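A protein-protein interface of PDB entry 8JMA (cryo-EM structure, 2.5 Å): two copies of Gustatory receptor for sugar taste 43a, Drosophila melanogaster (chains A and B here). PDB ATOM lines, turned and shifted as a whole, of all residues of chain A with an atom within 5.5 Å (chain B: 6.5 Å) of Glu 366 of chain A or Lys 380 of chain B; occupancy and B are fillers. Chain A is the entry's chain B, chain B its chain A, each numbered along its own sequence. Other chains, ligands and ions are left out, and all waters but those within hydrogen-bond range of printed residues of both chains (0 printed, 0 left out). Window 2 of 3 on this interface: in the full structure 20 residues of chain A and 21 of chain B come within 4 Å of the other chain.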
ATOM      1  N   ILE A 361     -23.706 -11.777 -33.666  1.00  0.00           N
ATOM      2  CA  ILE A 361     -23.237 -10.695 -34.525  1.00  0.00           C
ATOM      3  C   ILE A 361     -22.473  -9.667 -33.703  1.00  0.00           C
ATOM      4  O   ILE A 361     -21.425  -9.164 -34.126  1.00  0.00           O
ATOM      5  CB  ILE A 361     -24.415 -10.048 -35.275  1.00  0.00           C
ATOM      6  CG1 ILE A 361     -25.216 -11.105 -36.039  1.00  0.00           C
ATOM      7  CG2 ILE A 361     -23.904  -8.983 -36.232  1.00  0.00           C
ATOM      8  CD1 ILE A 361     -26.470 -10.568 -36.680  1.00  0.00           C
ATOM      9  N   VAL A 362     -22.988  -9.333 -32.519  1.00  0.00           N
ATOM     10  CA  VAL A 362     -22.320  -8.347 -31.680  1.00  0.00           C
ATOM     11  C   VAL A 362     -20.988  -8.887 -31.174  1.00  0.00           C
ATOM     12  O   VAL A 362     -20.018  -8.138 -31.036  1.00  0.00           O
ATOM     13  CB  VAL A 362     -23.239  -7.921 -30.523  1.00  0.00           C
ATOM     14  CG1 VAL A 362     -22.436  -7.239 -29.428  1.00  0.00           C
ATOM     15  CG2 VAL A 362     -24.327  -6.999 -31.040  1.00  0.00           C
ATOM     16  N   CYS A 363     -20.919 -10.186 -30.880  1.00  0.00           N
ATOM     17  CA  CYS A 363     -19.648 -10.779 -30.479  1.00  0.00           C
ATOM     18  C   CYS A 363     -18.625 -10.687 -31.601  1.00  0.00           C
ATOM     19  O   CYS A 363     -17.457 -10.356 -31.365  1.00  0.00           O
ATOM     20  CB  CYS A 363     -19.857 -12.235 -30.071  1.00  0.00           C
ATOM     21  SG  CYS A 363     -20.378 -12.459 -28.363  1.00  0.00           S
ATOM     22  N   GLU A 364     -19.045 -10.972 -32.835  1.00  0.00           N
ATOM     23  CA  GLU A 364     -18.125 -10.852 -33.960  1.00  0.00           C
ATOM     24  C   GLU A 364     -17.679  -9.408 -34.153  1.00  0.00           C
ATOM     25  O   GLU A 364     -16.504  -9.144 -34.434  1.00  0.00           O
ATOM     26  CB  GLU A 364     -18.776 -11.396 -35.230  1.00  0.00           C
ATOM     27  CG  GLU A 364     -18.491 -12.871 -35.462  1.00  0.00           C
ATOM     28  CD  GLU A 364     -19.258 -13.443 -36.636  1.00  0.00           C
ATOM     29  OE1 GLU A 364     -18.978 -13.037 -37.784  1.00  0.00           O
ATOM     30  OE2 GLU A 364     -20.137 -14.301 -36.410  1.00  0.00           O
ATOM     31  N   ILE A 365     -18.600  -8.456 -34.006  1.00  0.00           N
ATOM     32  CA  ILE A 365     -18.224  -7.050 -34.133  1.00  0.00           C
ATOM     33  C   ILE A 365     -17.223  -6.671 -33.046  1.00  0.00           C
ATOM     34  O   ILE A 365     -16.227  -5.991 -33.313  1.00  0.00           O
ATOM     35  CB  ILE A 365     -19.477  -6.158 -34.098  1.00  0.00           C
ATOM     36  CG1 ILE A 365     -20.301  -6.366 -35.368  1.00  0.00           C
ATOM     37  CG2 ILE A 365     -19.085  -4.696 -33.962  1.00  0.00           C
ATOM     38  CD1 ILE A 365     -21.697  -5.795 -35.296  1.00  0.00           C
ATOM     39  N   GLU A 366     -17.466  -7.109 -31.809  1.00  0.00           N
ATOM     40  CA  GLU A 366     -16.496  -6.915 -30.737  1.00  0.00           C
ATOM     41  C   GLU A 366     -15.132  -7.448 -31.146  1.00  0.00           C
ATOM     42  O   GLU A 366     -14.105  -6.783 -30.971  1.00  0.00           O
ATOM     43  CB  GLU A 366     -16.968  -7.622 -29.464  1.00  0.00           C
ATOM     44  CG  GLU A 366     -17.803  -6.773 -28.527  1.00  0.00           C
ATOM     45  CD  GLU A 366     -17.708  -7.224 -27.078  1.00  0.00           C
ATOM     46  OE1 GLU A 366     -17.150  -8.312 -26.820  1.00  0.00           O
ATOM     47  OE2 GLU A 366     -18.192  -6.489 -26.194  1.00  0.00           O
ATOM     48  N   ARG A 367     -15.109  -8.662 -31.695  1.00  0.00           N
ATOM     49  CA  ARG A 367     -13.869  -9.274 -32.148  1.00  0.00           C
ATOM     50  C   ARG A 367     -13.252  -8.551 -33.338  1.00  0.00           C
ATOM     51  O   ARG A 367     -12.082  -8.797 -33.647  1.00  0.00           O
ATOM     52  CB  ARG A 367     -14.124 -10.736 -32.514  1.00  0.00           C
ATOM     53  CG  ARG A 367     -12.981 -11.668 -32.179  1.00  0.00           C
ATOM     54  CD  ARG A 367     -13.448 -13.107 -32.062  1.00  0.00           C
ATOM     55  NE  ARG A 367     -14.287 -13.517 -33.184  1.00  0.00           N
ATOM     56  CZ  ARG A 367     -14.378 -14.760 -33.639  1.00  0.00           C
ATOM     57  NH1 ARG A 367     -13.692 -15.751 -33.092  1.00  0.00           N
ATOM     58  NH2 ARG A 367     -15.175 -15.015 -34.672  1.00  0.00           N
ATOM     59  N   LYS A 368     -13.998  -7.680 -34.012  1.00  0.00           N
ATOM     60  CA  LYS A 368     -13.532  -7.016 -35.225  1.00  0.00           C
ATOM     61  C   LYS A 368     -13.790  -5.513 -35.167  1.00  0.00           C
ATOM     62  O   LYS A 368     -14.268  -4.911 -36.132  1.00  0.00           O
ATOM     63  CB  LYS A 368     -14.199  -7.630 -36.452  1.00  0.00           C
ATOM     64  CG  LYS A 368     -13.634  -7.172 -37.787  1.00  0.00           C
ATOM     65  CD  LYS A 368     -14.746  -6.896 -38.795  1.00  0.00           C
ATOM     66  CE  LYS A 368     -15.085  -5.416 -38.894  1.00  0.00           C
ATOM     67  NZ  LYS A 368     -15.435  -5.023 -40.287  1.00  0.00           N
ATOM     68  N   VAL A 369     -13.472  -4.878 -34.040  1.00  0.00           N
ATOM     69  CA  VAL A 369     -13.665  -3.441 -33.869  1.00  0.00           C
ATOM     70  C   VAL A 369     -12.517  -2.888 -33.035  1.00  0.00           C
ATOM     71  O   VAL A 369     -12.013  -3.561 -32.130  1.00  0.00           O
ATOM     72  CB  VAL A 369     -15.023  -3.122 -33.209  1.00  0.00           C
ATOM     73  CG1 VAL A 369     -14.941  -3.297 -31.698  1.00  0.00           C
ATOM     74  CG2 VAL A 369     -15.471  -1.715 -33.563  1.00  0.00           C
ATOM     75  N   VAL A 378     -20.224  -1.060 -28.956  1.00  0.00           N
ATOM     76  CA  VAL A 378     -20.410  -2.496 -29.121  1.00  0.00           C
ATOM     77  C   VAL A 378     -20.368  -3.198 -27.769  1.00  0.00           C
ATOM     78  O   VAL A 378     -21.095  -4.170 -27.540  1.00  0.00           O
ATOM     79  CB  VAL A 378     -19.362  -3.065 -30.092  1.00  0.00           C
ATOM     80  CG1 VAL A 378     -19.558  -4.561 -30.267  1.00  0.00           C
ATOM     81  CG2 VAL A 378     -19.456  -2.375 -31.441  1.00  0.00           C
ATOM     82  N   LYS A 379     -19.509  -2.737 -26.860  1.00  0.00           N
ATOM     83  CA  LYS A 379     -19.479  -3.319 -25.523  1.00  0.00           C
ATOM     84  C   LYS A 379     -20.812  -3.115 -24.814  1.00  0.00           C
ATOM     85  O   LYS A 379     -21.324  -4.027 -24.156  1.00  0.00           O
ATOM     86  CB  LYS A 379     -18.334  -2.706 -24.716  1.00  0.00           C
ATOM     87  CG  LYS A 379     -18.297  -3.097 -23.238  1.00  0.00           C
ATOM     88  CD  LYS A 379     -18.442  -4.600 -23.007  1.00  0.00           C
ATOM     89  CE  LYS A 379     -17.327  -5.408 -23.657  1.00  0.00           C
ATOM     90  NZ  LYS A 379     -17.775  -6.787 -23.981  1.00  0.00           N
ATOM     91  N   TRP A 382     -23.340  -5.513 -26.315  1.00  0.00           N
ATOM     92  CA  TRP A 382     -23.123  -6.862 -25.801  1.00  0.00           C
ATOM     93  C   TRP A 382     -23.666  -7.000 -24.388  1.00  0.00           C
ATOM     94  O   TRP A 382     -24.329  -7.992 -24.061  1.00  0.00           O
ATOM     95  CB  TRP A 382     -21.632  -7.195 -25.835  1.00  0.00           C
ATOM     96  CG  TRP A 382     -21.325  -8.639 -25.586  1.00  0.00           C
ATOM     97  CD1 TRP A 382     -21.282  -9.638 -26.512  1.00  0.00           C
ATOM     98  CD2 TRP A 382     -21.010  -9.246 -24.327  1.00  0.00           C
ATOM     99  NE1 TRP A 382     -20.967 -10.829 -25.909  1.00  0.00           N
ATOM    100  CE2 TRP A 382     -20.797 -10.616 -24.567  1.00  0.00           C
ATOM    101  CE3 TRP A 382     -20.894  -8.765 -23.021  1.00  0.00           C
ATOM    102  CZ2 TRP A 382     -20.470 -11.509 -23.551  1.00  0.00           C
ATOM    103  CZ3 TRP A 382     -20.572  -9.654 -22.013  1.00  0.00           C
ATOM    104  CH2 TRP A 382     -20.363 -11.010 -22.284  1.00  0.00           C
ATOM    105  N   ALA B 275      -9.360 -19.834 -31.154  1.00  0.00           N
ATOM    106  CA  ALA B 275     -10.655 -19.210 -30.905  1.00  0.00           C
ATOM    107  C   ALA B 275     -11.511 -19.184 -32.165  1.00  0.00           C
ATOM    108  O   ALA B 275     -12.713 -19.483 -32.117  1.00  0.00           O
ATOM    109  CB  ALA B 275     -10.461 -17.797 -30.361  1.00  0.00           C
ATOM    110  N   GLU B 366      -6.784 -17.951 -18.297  1.00  0.00           N
ATOM    111  CA  GLU B 366      -6.964 -16.629 -17.708  1.00  0.00           C
ATOM    112  C   GLU B 366      -6.304 -16.556 -16.339  1.00  0.00           C
ATOM    113  O   GLU B 366      -5.581 -15.605 -16.027  1.00  0.00           O
ATOM    114  CB  GLU B 366      -8.456 -16.307 -17.581  1.00  0.00           C
ATOM    115  CG  GLU B 366      -9.063 -15.590 -18.769  1.00  0.00           C
ATOM    116  CD  GLU B 366     -10.269 -14.744 -18.394  1.00  0.00           C
ATOM    117  OE1 GLU B 366     -10.757 -14.861 -17.250  1.00  0.00           O
ATOM    118  OE2 GLU B 366     -10.733 -13.958 -19.246  1.00  0.00           O
ATOM    119  N   ALA B 375      -2.999 -11.980 -22.607  1.00  0.00           N
ATOM    120  CA  ALA B 375      -4.102 -11.823 -21.666  1.00  0.00           C
ATOM    121  C   ALA B 375      -5.337 -11.266 -22.359  1.00  0.00           C
ATOM    122  O   ALA B 375      -6.460 -11.709 -22.095  1.00  0.00           O
ATOM    123  CB  ALA B 375      -3.683 -10.920 -20.508  1.00  0.00           C
ATOM    124  N   GLU B 376      -5.153 -10.292 -23.253  1.00  0.00           N
ATOM    125  CA  GLU B 376      -6.289  -9.763 -24.000  1.00  0.00           C
ATOM    126  C   GLU B 376      -6.899 -10.832 -24.898  1.00  0.00           C
ATOM    127  O   GLU B 376      -8.126 -10.927 -25.022  1.00  0.00           O
ATOM    128  CB  GLU B 376      -5.851  -8.551 -24.823  1.00  0.00           C
ATOM    129  CG  GLU B 376      -6.934  -7.965 -25.722  1.00  0.00           C
ATOM    130  CD  GLU B 376      -8.038  -7.282 -24.943  1.00  0.00           C
ATOM    131  OE1 GLU B 376      -8.069  -7.419 -23.703  1.00  0.00           O
ATOM    132  OE2 GLU B 376      -8.876  -6.601 -25.572  1.00  0.00           O
ATOM    133  N   ALA B 377      -6.056 -11.641 -25.545  1.00  0.00           N
ATOM    134  CA  ALA B 377      -6.570 -12.709 -26.394  1.00  0.00           C
ATOM    135  C   ALA B 377      -7.393 -13.701 -25.586  1.00  0.00           C
ATOM    136  O   ALA B 377      -8.471 -14.128 -26.020  1.00  0.00           O
ATOM    137  CB  ALA B 377      -5.413 -13.421 -27.095  1.00  0.00           C
ATOM    138  N   VAL B 378      -6.908 -14.073 -24.403  1.00  0.00           N
ATOM    139  CA  VAL B 378      -7.641 -15.023 -23.575  1.00  0.00           C
ATOM    140  C   VAL B 378      -8.937 -14.401 -23.071  1.00  0.00           C
ATOM    141  O   VAL B 378      -9.961 -15.082 -22.955  1.00  0.00           O
ATOM    142  CB  VAL B 378      -6.758 -15.519 -22.417  1.00  0.00           C
ATOM    143  CG1 VAL B 378      -7.522 -16.511 -21.556  1.00  0.00           C
ATOM    144  CG2 VAL B 378      -5.496 -16.169 -22.952  1.00  0.00           C
ATOM    145  N   LYS B 379      -8.917 -13.109 -22.744  1.00  0.00           N
ATOM    146  CA  LYS B 379     -10.145 -12.441 -22.329  1.00  0.00           C
ATOM    147  C   LYS B 379     -11.174 -12.455 -23.453  1.00  0.00           C
ATOM    148  O   LYS B 379     -12.363 -12.698 -23.218  1.00  0.00           O
ATOM    149  CB  LYS B 379      -9.836 -11.008 -21.893  1.00  0.00           C
ATOM    150  CG  LYS B 379     -11.057 -10.138 -21.601  1.00  0.00           C
ATOM    151  CD  LYS B 379     -12.084 -10.820 -20.698  1.00  0.00           C
ATOM    152  CE  LYS B 379     -11.519 -11.179 -19.330  1.00  0.00           C
ATOM    153  NZ  LYS B 379     -12.237 -12.336 -18.734  1.00  0.00           N
ATOM    154  N   LYS B 380     -10.730 -12.199 -24.684  1.00  0.00           N
ATOM    155  CA  LYS B 380     -11.637 -12.257 -25.824  1.00  0.00           C
ATOM    156  C   LYS B 380     -12.193 -13.662 -26.015  1.00  0.00           C
ATOM    157  O   LYS B 380     -13.389 -13.834 -26.285  1.00  0.00           O
ATOM    158  CB  LYS B 380     -10.914 -11.791 -27.087  1.00  0.00           C
ATOM    159  CG  LYS B 380     -10.792 -10.284 -27.199  1.00  0.00           C
ATOM    160  CD  LYS B 380      -9.783  -9.884 -28.265  1.00  0.00           C
ATOM    161  CE  LYS B 380     -10.371  -8.893 -29.262  1.00  0.00           C
ATOM    162  NZ  LYS B 380     -11.056  -7.741 -28.605  1.00  0.00           N
ATOM    163  N   PHE B 381     -11.341 -14.681 -25.885  1.00  0.00           N
ATOM    164  CA  PHE B 381     -11.809 -16.058 -26.020  1.00  0.00           C
ATOM    165  C   PHE B 381     -12.846 -16.390 -24.953  1.00  0.00           C
ATOM    166  O   PHE B 381     -13.853 -17.049 -25.239  1.00  0.00           O
ATOM    167  CB  PHE B 381     -10.622 -17.021 -25.937  1.00  0.00           C
ATOM    168  CG  PHE B 381     -10.865 -18.373 -26.573  1.00  0.00           C
ATOM    169  CD1 PHE B 381     -12.111 -18.733 -27.060  1.00  0.00           C
ATOM    170  CD2 PHE B 381      -9.831 -19.286 -26.678  1.00  0.00           C
ATOM    171  CE1 PHE B 381     -12.315 -19.972 -27.638  1.00  0.00           C
ATOM    172  CE2 PHE B 381     -10.031 -20.525 -27.255  1.00  0.00           C
ATOM    173  CZ  PHE B 381     -11.275 -20.867 -27.735  1.00  0.00           C
ATOM    174  N   TRP B 382     -12.608 -15.958 -23.713  1.00  0.00           N
ATOM    175  CA  TRP B 382     -13.576 -16.187 -22.645  1.00  0.00           C
ATOM    176  C   TRP B 382     -14.899 -15.504 -22.952  1.00  0.00           C
ATOM    177  O   TRP B 382     -15.970 -16.096 -22.777  1.00  0.00           O
ATOM    178  CB  TRP B 382     -13.011 -15.684 -21.317  1.00  0.00           C
ATOM    179  CG  TRP B 382     -13.801 -16.109 -20.119  1.00  0.00           C
ATOM    180  CD1 TRP B 382     -13.660 -17.269 -19.417  1.00  0.00           C
ATOM    181  CD2 TRP B 382     -14.851 -15.377 -19.477  1.00  0.00           C
ATOM    182  NE1 TRP B 382     -14.560 -17.307 -18.382  1.00  0.00           N
ATOM    183  CE2 TRP B 382     -15.305 -16.158 -18.398  1.00  0.00           C
ATOM    184  CE3 TRP B 382     -15.455 -14.140 -19.713  1.00  0.00           C
ATOM    185  CZ2 TRP B 382     -16.331 -15.741 -17.555  1.00  0.00           C
ATOM    186  CZ3 TRP B 382     -16.475 -13.729 -18.877  1.00  0.00           C
ATOM    187  CH2 TRP B 382     -16.902 -14.527 -17.811  1.00  0.00           C
ATOM    188  N   GLN B 383     -14.846 -14.252 -23.410  1.00  0.00           N
ATOM    189  CA  GLN B 383     -16.067 -13.556 -23.799  1.00  0.00           C
ATOM    190  C   GLN B 383     -16.819 -14.342 -24.862  1.00  0.00           C
ATOM    191  O   GLN B 383     -18.041 -14.513 -24.784  1.00  0.00           O
ATOM    192  CB  GLN B 383     -15.727 -12.160 -24.319  1.00  0.00           C
ATOM    193  CG  GLN B 383     -15.161 -11.224 -23.277  1.00  0.00           C
ATOM    194  CD  GLN B 383     -16.237 -10.555 -22.462  1.00  0.00           C
ATOM    195  OE1 GLN B 383     -16.996 -11.216 -21.756  1.00  0.00           O
ATOM    196  NE2 GLN B 383     -16.317  -9.236 -22.560  1.00  0.00           N
ATOM    197  N   GLN B 384     -16.093 -14.829 -25.867  1.00  0.00           N
ATOM    198  CA  GLN B 384     -16.710 -15.588 -26.948  1.00  0.00           C
ATOM    199  C   GLN B 384     -17.397 -16.836 -26.411  1.00  0.00           C
ATOM    200  O   GLN B 384     -18.573 -17.086 -26.695  1.00  0.00           O
ATOM    201  CB  GLN B 384     -15.639 -15.943 -27.977  1.00  0.00           C
ATOM    202  CG  GLN B 384     -16.085 -16.819 -29.126  1.00  0.00           C
ATOM    203  CD  GLN B 384     -14.910 -17.383 -29.893  1.00  0.00           C
ATOM    204  OE1 GLN B 384     -13.952 -16.672 -30.190  1.00  0.00           O
ATOM    205  NE2 GLN B 384     -14.970 -18.668 -30.210  1.00  0.00           N
ATOM    206  N   LEU B 385     -16.678 -17.622 -25.612  1.00  0.00           N
ATOM    207  CA  LEU B 385     -17.219 -18.867 -25.084  1.00  0.00           C
ATOM    208  C   LEU B 385     -18.356 -18.643 -24.099  1.00  0.00           C
ATOM    209  O   LEU B 385     -19.142 -19.563 -23.860  1.00  0.00           O
ATOM    210  CB  LEU B 385     -16.107 -19.663 -24.411  1.00  0.00           C
ATOM    211  CG  LEU B 385     -14.955 -20.094 -25.309  1.00  0.00           C
ATOM    212  CD1 LEU B 385     -13.795 -20.571 -24.470  1.00  0.00           C
ATOM    213  CD2 LEU B 385     -15.407 -21.171 -26.263  1.00  0.00           C
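Glu 366 of chain A touches one residue of chain B.
Lys 380 of chain B touches just one residue of chain A: Glu 366 (3.98 Å).
Of the printed residues of chain B, Arg 367 of chain A touches Ala 275 and Gln 384.
Printed residues of chain B within 4 Å of Trp 382 of chain A: Gln 383.
Val 369 of chain A touches none of the printed residues of chain B.
The nearest residue of chain B that does not touch Glu 366 of chain A is Gln 383 of chain B (4.4 Å).
The nearest printed residue of chain A that does not touch Ala 275 of chain B is Glu 364 of chain A (9.4 Å).
NE2 of Gln 383 of chain B sits close to NZ of Lys 379 of chain A, 3.2 Å away.
NH1 of Arg 367 of chain A lies within hydrogen-bond range of OE1 of Gln 384 of chain B, 3.1 Å away.
SG of Cys 363 of chain A sits at hydrogen-bond distance from NE1 of Trp 382 of chain A, at 3.0 Å.
OE2 of Glu 376 of chain B lies within salt-bridge range of NZ of Lys 380 of chain B.
The side-chain amide nitrogen (NE2) of Gln 384 of chain B sits at hydrogen-bond distance from the backbone carbonyl oxygen (O) of Ala 275 of chain B (3.1 Å).
OE1 of Glu 366 of chain A is in salt-bridge range of NZ of Lys 379 of chain A.
NZ of Lys 380 of chain B touches O of Glu 366 of chain A, at 3.98 Å.
O of Ala 275 of chain B touches NH1 of Arg 367 of chain A (3.98 Å).
Gln 383 of chain B touches Trp 382 of chain A.
Positions printed for both chains: 366, 378, 379 and 382.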
